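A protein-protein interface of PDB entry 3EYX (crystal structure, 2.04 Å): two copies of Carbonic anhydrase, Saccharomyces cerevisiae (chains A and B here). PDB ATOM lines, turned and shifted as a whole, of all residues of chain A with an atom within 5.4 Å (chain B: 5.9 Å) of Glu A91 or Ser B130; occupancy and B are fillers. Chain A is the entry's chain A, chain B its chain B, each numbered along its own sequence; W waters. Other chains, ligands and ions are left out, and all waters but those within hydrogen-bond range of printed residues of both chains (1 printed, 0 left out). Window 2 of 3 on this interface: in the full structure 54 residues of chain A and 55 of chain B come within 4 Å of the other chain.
OE1 of Glu A91 lies within hydrogen-bond range of N of Leu B132, at 3.0 Å.
The side-chain carboxylate (OE2) of Glu A91 lies within hydrogen-bond range of a ring nitrogen (ND1) of His B131 (2.7 Å).
The backbone carbonyl oxygen (O) of Leu B124 is in hydrogen-bond range of the backbone NH (N) of Cys B129, at 2.9 Å.
Among the printed residues, pairs that only touch across the chains: Glu A91 with Cys B129, Ile A95 with Asn B128, Ala A88 with Tyr B135, Glu A91 with Ser B130, Ile A95 with Cys B129, Lys A87 with His B131, Glu A91 with Asn B128, Phe A92 with Leu B132, Ala A88 with Leu B132 and Ala A88 with His B131.
Of chain B, only Asn B128 (3.7 Å), Cys B129 (3.2 Å), Ser B130 (3.6 Å), His B131 (2.7 Å) and Leu B132 (3.0 Å) come within 4 Å of Glu A91.
Of chain A, only Glu A91 comes within 4 Å of Ser B130.
Of the printed residues of chain A, Tyr B135 touches Ala A88.
Of the printed residues of chain B, Phe A92 touches Leu B132 (3.7 Å).
Ala A93 touches none of the printed residues of chain B.
Hydrophobic or aromatic side chains of chain B within 4 Å of the printed part of chain A: His B131, Leu B132 and Tyr B135.
Of the 12 printed residues of chain A, 5 touch a printed residue of chain B.
Among the printed residues, 12 pairs touch across the chains.
No position is printed for both chains.
Water W1 bridges the side-chain hydroxyl of Thr A180 and the backbone carbonyl oxygen of Asn B128.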
ATOM      1  N   LEU A  86     -13.771  18.319 -29.609  1.00  0.00           N
ATOM      2  CA  LEU A  86     -14.528  19.529 -29.936  1.00  0.00           C
ATOM      3  C   LEU A  86     -14.943  20.301 -28.688  1.00  0.00           C
ATOM      4  O   LEU A  86     -14.671  21.501 -28.579  1.00  0.00           O
ATOM      5  CB  LEU A  86     -15.772  19.207 -30.762  1.00  0.00           C
ATOM      6  CG  LEU A  86     -16.714  20.397 -31.028  1.00  0.00           C
ATOM      7  CD1 LEU A  86     -16.089  21.435 -31.952  1.00  0.00           C
ATOM      8  CD2 LEU A  86     -18.053  19.946 -31.578  1.00  0.00           C
ATOM      9  N   LYS A  87     -15.614  19.608 -27.765  1.00  0.00           N
ATOM     10  CA  LYS A  87     -16.087  20.211 -26.529  1.00  0.00           C
ATOM     11  C   LYS A  87     -14.928  20.733 -25.688  1.00  0.00           C
ATOM     12  O   LYS A  87     -14.979  21.861 -25.234  1.00  0.00           O
ATOM     13  CB  LYS A  87     -16.950  19.228 -25.735  1.00  0.00           C
ATOM     14  CG  LYS A  87     -18.340  19.010 -26.335  1.00  0.00           C
ATOM     15  CD  LYS A  87     -19.153  18.041 -25.493  1.00  0.00           C
ATOM     16  CE  LYS A  87     -20.628  18.075 -25.877  1.00  0.00           C
ATOM     17  NZ  LYS A  87     -21.402  17.085 -25.080  1.00  0.00           N
ATOM     18  N   ALA A  88     -13.900  19.906 -25.492  1.00  0.00           N
ATOM     19  CA  ALA A  88     -12.662  20.307 -24.824  1.00  0.00           C
ATOM     20  C   ALA A  88     -11.977  21.531 -25.462  1.00  0.00           C
ATOM     21  O   ALA A  88     -11.564  22.457 -24.767  1.00  0.00           O
ATOM     22  CB  ALA A  88     -11.690  19.142 -24.787  1.00  0.00           C
ATOM     23  N   THR A  89     -11.855  21.513 -26.783  1.00  0.00           N
ATOM     24  CA  THR A  89     -11.230  22.617 -27.536  1.00  0.00           C
ATOM     25  C   THR A  89     -12.037  23.923 -27.456  1.00  0.00           C
ATOM     26  O   THR A  89     -11.461  25.000 -27.281  1.00  0.00           O
ATOM     27  CB  THR A  89     -10.955  22.194 -29.019  1.00  0.00           C
ATOM     28  OG1 THR A  89     -10.244  20.944 -29.022  1.00  0.00           O
ATOM     29  CG2 THR A  89     -10.131  23.257 -29.786  1.00  0.00           C
ATOM     30  N   LEU A  90     -13.359  23.832 -27.581  1.00  0.00           N
ATOM     31  CA  LEU A  90     -14.209  25.033 -27.472  1.00  0.00           C
ATOM     32  C   LEU A  90     -14.164  25.607 -26.050  1.00  0.00           C
ATOM     33  O   LEU A  90     -14.029  26.818 -25.869  1.00  0.00           O
ATOM     34  CB  LEU A  90     -15.654  24.761 -27.925  1.00  0.00           C
ATOM     35  CG  LEU A  90     -15.866  24.439 -29.415  1.00  0.00           C
ATOM     36  CD1 LEU A  90     -17.280  23.992 -29.655  1.00  0.00           C
ATOM     37  CD2 LEU A  90     -15.516  25.636 -30.325  1.00  0.00           C
ATOM     38  N   GLU A  91     -14.244  24.730 -25.051  1.00  0.00           N
ATOM     39  CA  GLU A  91     -14.135  25.152 -23.651  1.00  0.00           C
ATOM     40  C   GLU A  91     -12.811  25.853 -23.349  1.00  0.00           C
ATOM     41  O   GLU A  91     -12.806  26.954 -22.805  1.00  0.00           O
ATOM     42  CB  GLU A  91     -14.370  23.975 -22.703  1.00  0.00           C
ATOM     43  CG  GLU A  91     -15.850  23.627 -22.560  1.00  0.00           C
ATOM     44  CD  GLU A  91     -16.090  22.193 -22.120  1.00  0.00           C
ATOM     45  OE1 GLU A  91     -15.184  21.597 -21.513  1.00  0.00           O
ATOM     46  OE2 GLU A  91     -17.187  21.672 -22.382  1.00  0.00           O
ATOM     47  N   PHE A  92     -11.698  25.236 -23.738  1.00  0.00           N
ATOM     48  CA  PHE A  92     -10.388  25.861 -23.568  1.00  0.00           C
ATOM     49  C   PHE A  92     -10.260  27.218 -24.276  1.00  0.00           C
ATOM     50  O   PHE A  92      -9.920  28.217 -23.641  1.00  0.00           O
ATOM     51  CB  PHE A  92      -9.255  24.921 -23.993  1.00  0.00           C
ATOM     52  CG  PHE A  92      -7.900  25.462 -23.684  1.00  0.00           C
ATOM     53  CD1 PHE A  92      -7.555  25.784 -22.376  1.00  0.00           C
ATOM     54  CD2 PHE A  92      -6.984  25.697 -24.698  1.00  0.00           C
ATOM     55  CE1 PHE A  92      -6.307  26.322 -22.077  1.00  0.00           C
ATOM     56  CE2 PHE A  92      -5.726  26.227 -24.405  1.00  0.00           C
ATOM     57  CZ  PHE A  92      -5.394  26.544 -23.093  1.00  0.00           C
ATOM     58  N   ALA A  93     -10.524  27.248 -25.580  1.00  0.00           N
ATOM     59  CA  ALA A  93     -10.453  28.497 -26.367  1.00  0.00           C
ATOM     60  C   ALA A  93     -11.309  29.623 -25.774  1.00  0.00           C
ATOM     61  O   ALA A  93     -10.822  30.731 -25.546  1.00  0.00           O
ATOM     62  CB  ALA A  93     -10.838  28.242 -27.827  1.00  0.00           C
ATOM     63  N   ILE A  94     -12.570  29.317 -25.487  1.00  0.00           N
ATOM     64  CA  ILE A  94     -13.533  30.336 -25.066  1.00  0.00           C
ATOM     65  C   ILE A  94     -13.368  30.730 -23.596  1.00  0.00           C
ATOM     66  O   ILE A  94     -13.241  31.914 -23.281  1.00  0.00           O
ATOM     67  CB  ILE A  94     -14.987  29.912 -25.381  1.00  0.00           C
ATOM     68  CG1 ILE A  94     -15.185  29.813 -26.902  1.00  0.00           C
ATOM     69  CG2 ILE A  94     -15.986  30.884 -24.749  1.00  0.00           C
ATOM     70  CD1 ILE A  94     -16.273  28.820 -27.362  1.00  0.00           C
ATOM     71  N   ILE A  95     -13.342  29.739 -22.708  1.00  0.00           N
ATOM     72  CA  ILE A  95     -13.383  30.015 -21.282  1.00  0.00           C
ATOM     73  C   ILE A  95     -12.002  30.316 -20.702  1.00  0.00           C
ATOM     74  O   ILE A  95     -11.872  31.200 -19.860  1.00  0.00           O
ATOM     75  CB  ILE A  95     -14.108  28.875 -20.498  1.00  0.00           C
ATOM     76  CG1 ILE A  95     -15.555  28.725 -20.999  1.00  0.00           C
ATOM     77  CG2 ILE A  95     -14.051  29.104 -18.966  1.00  0.00           C
ATOM     78  CD1 ILE A  95     -16.292  27.500 -20.447  1.00  0.00           C
ATOM     79  N   CYS A  96     -10.981  29.585 -21.141  1.00  0.00           N
ATOM     80  CA  CYS A  96      -9.652  29.717 -20.559  1.00  0.00           C
ATOM     81  C   CYS A  96      -8.788  30.728 -21.319  1.00  0.00           C
ATOM     82  O   CYS A  96      -8.250  31.650 -20.713  1.00  0.00           O
ATOM     83  CB  CYS A  96      -8.958  28.348 -20.465  1.00  0.00           C
ATOM     84  SG  CYS A  96      -9.900  27.082 -19.548  1.00  0.00           S
ATOM     85  N   THR A 180     -21.304  26.202 -24.658  1.00  0.00           N
ATOM     86  CA  THR A 180     -20.185  27.119 -24.403  1.00  0.00           C
ATOM     87  C   THR A 180     -20.182  28.274 -25.417  1.00  0.00           C
ATOM     88  O   THR A 180     -19.938  29.432 -25.052  1.00  0.00           O
ATOM     89  CB  THR A 180     -18.819  26.368 -24.433  1.00  0.00           C
ATOM     90  OG1 THR A 180     -18.885  25.215 -23.589  1.00  0.00           O
ATOM     91  CG2 THR A 180     -17.675  27.267 -23.944  1.00  0.00           C
ATOM     92  N   LEU B 124     -11.388  22.897 -13.310  1.00  0.00           N
ATOM     93  CA  LEU B 124     -12.045  23.005 -14.616  1.00  0.00           C
ATOM     94  C   LEU B 124     -13.567  22.754 -14.603  1.00  0.00           C
ATOM     95  O   LEU B 124     -14.306  23.485 -15.256  1.00  0.00           O
ATOM     96  CB  LEU B 124     -11.312  22.164 -15.692  1.00  0.00           C
ATOM     97  CG  LEU B 124     -10.102  22.752 -16.454  1.00  0.00           C
ATOM     98  CD1 LEU B 124      -9.178  23.545 -15.567  1.00  0.00           C
ATOM     99  CD2 LEU B 124      -9.299  21.676 -17.183  1.00  0.00           C
ATOM    100  N   PRO B 125     -14.044  21.718 -13.876  1.00  0.00           N
ATOM    101  CA  PRO B 125     -15.510  21.529 -13.765  1.00  0.00           C
ATOM    102  C   PRO B 125     -16.287  22.750 -13.217  1.00  0.00           C
ATOM    103  O   PRO B 125     -17.398  23.035 -13.692  1.00  0.00           O
ATOM    104  CB  PRO B 125     -15.642  20.330 -12.818  1.00  0.00           C
ATOM    105  CG  PRO B 125     -14.357  19.574 -13.005  1.00  0.00           C
ATOM    106  CD  PRO B 125     -13.307  20.644 -13.177  1.00  0.00           C
ATOM    107  N   ASN B 128     -17.138  25.367 -15.876  1.00  0.00           N
ATOM    108  CA  ASN B 128     -17.911  24.844 -16.991  1.00  0.00           C
ATOM    109  C   ASN B 128     -17.017  24.304 -18.121  1.00  0.00           C
ATOM    110  O   ASN B 128     -17.352  24.422 -19.302  1.00  0.00           O
ATOM    111  CB  ASN B 128     -18.922  25.902 -17.478  1.00  0.00           C
ATOM    112  CG  ASN B 128     -19.838  26.405 -16.356  1.00  0.00           C
ATOM    113  OD1 ASN B 128     -20.188  25.661 -15.440  1.00  0.00           O
ATOM    114  ND2 ASN B 128     -20.226  27.677 -16.429  1.00  0.00           N
ATOM    115  N   CYS B 129     -15.883  23.712 -17.725  1.00  0.00           N
ATOM    116  CA  CYS B 129     -14.926  23.063 -18.643  1.00  0.00           C
ATOM    117  C   CYS B 129     -14.709  21.576 -18.304  1.00  0.00           C
ATOM    118  O   CYS B 129     -13.574  21.096 -18.248  1.00  0.00           O
ATOM    119  CB  CYS B 129     -13.579  23.789 -18.611  1.00  0.00           C
ATOM    120  SG  CYS B 129     -13.600  25.495 -19.216  1.00  0.00           S
ATOM    121  N   SER B 130     -15.800  20.847 -18.091  1.00  0.00           N
ATOM    122  CA  SER B 130     -15.710  19.461 -17.648  1.00  0.00           C
ATOM    123  C   SER B 130     -15.193  18.553 -18.757  1.00  0.00           C
ATOM    124  O   SER B 130     -14.644  17.494 -18.487  1.00  0.00           O
ATOM    125  CB  SER B 130     -17.060  18.961 -17.098  1.00  0.00           C
ATOM    126  OG  SER B 130     -17.959  18.611 -18.135  1.00  0.00           O
ATOM    127  N   HIS B 131     -15.364  18.966 -20.004  1.00  0.00           N
ATOM    128  CA  HIS B 131     -14.837  18.181 -21.113  1.00  0.00           C
ATOM    129  C   HIS B 131     -13.333  18.400 -21.312  1.00  0.00           C
ATOM    130  O   HIS B 131     -12.596  17.452 -21.565  1.00  0.00           O
ATOM    131  CB  HIS B 131     -15.646  18.428 -22.385  1.00  0.00           C
ATOM    132  CG  HIS B 131     -17.104  18.160 -22.207  1.00  0.00           C
ATOM    133  ND1 HIS B 131     -18.044  19.164 -22.154  1.00  0.00           N
ATOM    134  CD2 HIS B 131     -17.774  17.000 -22.002  1.00  0.00           C
ATOM    135  CE1 HIS B 131     -19.235  18.632 -21.948  1.00  0.00           C
ATOM    136  NE2 HIS B 131     -19.098  17.321 -21.851  1.00  0.00           N
ATOM    137  N   LEU B 132     -12.874  19.641 -21.194  1.00  0.00           N
ATOM    138  CA  LEU B 132     -11.433  19.884 -21.128  1.00  0.00           C
ATOM    139  C   LEU B 132     -10.836  19.096 -19.962  1.00  0.00           C
ATOM    140  O   LEU B 132      -9.745  18.541 -20.076  1.00  0.00           O
ATOM    141  CB  LEU B 132     -11.118  21.371 -20.978  1.00  0.00           C
ATOM    142  CG  LEU B 132      -9.623  21.721 -20.867  1.00  0.00           C
ATOM    143  CD1 LEU B 132      -8.850  21.329 -22.155  1.00  0.00           C
ATOM    144  CD2 LEU B 132      -9.416  23.202 -20.516  1.00  0.00           C
ATOM    145  N   TYR B 133     -11.559  19.055 -18.841  1.00  0.00           N
ATOM    146  CA  TYR B 133     -11.128  18.268 -17.685  1.00  0.00           C
ATOM    147  C   TYR B 133     -10.887  16.805 -18.086  1.00  0.00           C
ATOM    148  O   TYR B 133      -9.820  16.244 -17.799  1.00  0.00           O
ATOM    149  CB  TYR B 133     -12.142  18.369 -16.524  1.00  0.00           C
ATOM    150  CG  TYR B 133     -11.807  17.462 -15.354  1.00  0.00           C
ATOM    151  CD1 TYR B 133     -10.906  17.874 -14.359  1.00  0.00           C
ATOM    152  CD2 TYR B 133     -12.363  16.187 -15.251  1.00  0.00           C
ATOM    153  CE1 TYR B 133     -10.572  17.032 -13.285  1.00  0.00           C
ATOM    154  CE2 TYR B 133     -12.030  15.341 -14.186  1.00  0.00           C
ATOM    155  CZ  TYR B 133     -11.145  15.782 -13.202  1.00  0.00           C
ATOM    156  OH  TYR B 133     -10.810  14.961 -12.144  1.00  0.00           O
ATOM    157  N   LYS B 134     -11.871  16.186 -18.734  1.00  0.00           N
ATOM    158  CA  LYS B 134     -11.738  14.776 -19.131  1.00  0.00           C
ATOM    159  C   LYS B 134     -10.640  14.585 -20.184  1.00  0.00           C
ATOM    160  O   LYS B 134      -9.857  13.643 -20.103  1.00  0.00           O
ATOM    161  CB  LYS B 134     -13.071  14.200 -19.631  1.00  0.00           C
ATOM    162  CG  LYS B 134     -13.031  12.685 -19.889  1.00  0.00           C
ATOM    163  CD  LYS B 134     -14.432  12.122 -20.145  1.00  0.00           C
ATOM    164  CE  LYS B 134     -14.378  10.657 -20.555  1.00  0.00           C
ATOM    165  NZ  LYS B 134     -15.763  10.090 -20.640  1.00  0.00           N
ATOM    166  N   TYR B 135     -10.586  15.499 -21.154  1.00  0.00           N
ATOM    167  CA  TYR B 135      -9.580  15.485 -22.228  1.00  0.00           C
ATOM    168  C   TYR B 135      -8.144  15.463 -21.701  1.00  0.00           C
ATOM    169  O   TYR B 135      -7.256  14.842 -22.298  1.00  0.00           O
ATOM    170  CB  TYR B 135      -9.778  16.713 -23.127  1.00  0.00           C
ATOM    171  CG  TYR B 135      -8.864  16.780 -24.329  1.00  0.00           C
ATOM    172  CD1 TYR B 135      -9.248  16.236 -25.552  1.00  0.00           C
ATOM    173  CD2 TYR B 135      -7.610  17.392 -24.242  1.00  0.00           C
ATOM    174  CE1 TYR B 135      -8.406  16.300 -26.664  1.00  0.00           C
ATOM    175  CE2 TYR B 135      -6.765  17.459 -25.336  1.00  0.00           C
ATOM    176  CZ  TYR B 135      -7.159  16.913 -26.543  1.00  0.00           C
ATOM    177  OH  TYR B 135      -6.300  16.976 -27.616  1.00  0.00           O
HETATM  178  O   HOH W   1     -19.177  25.519 -21.093  1.00  0.00           O
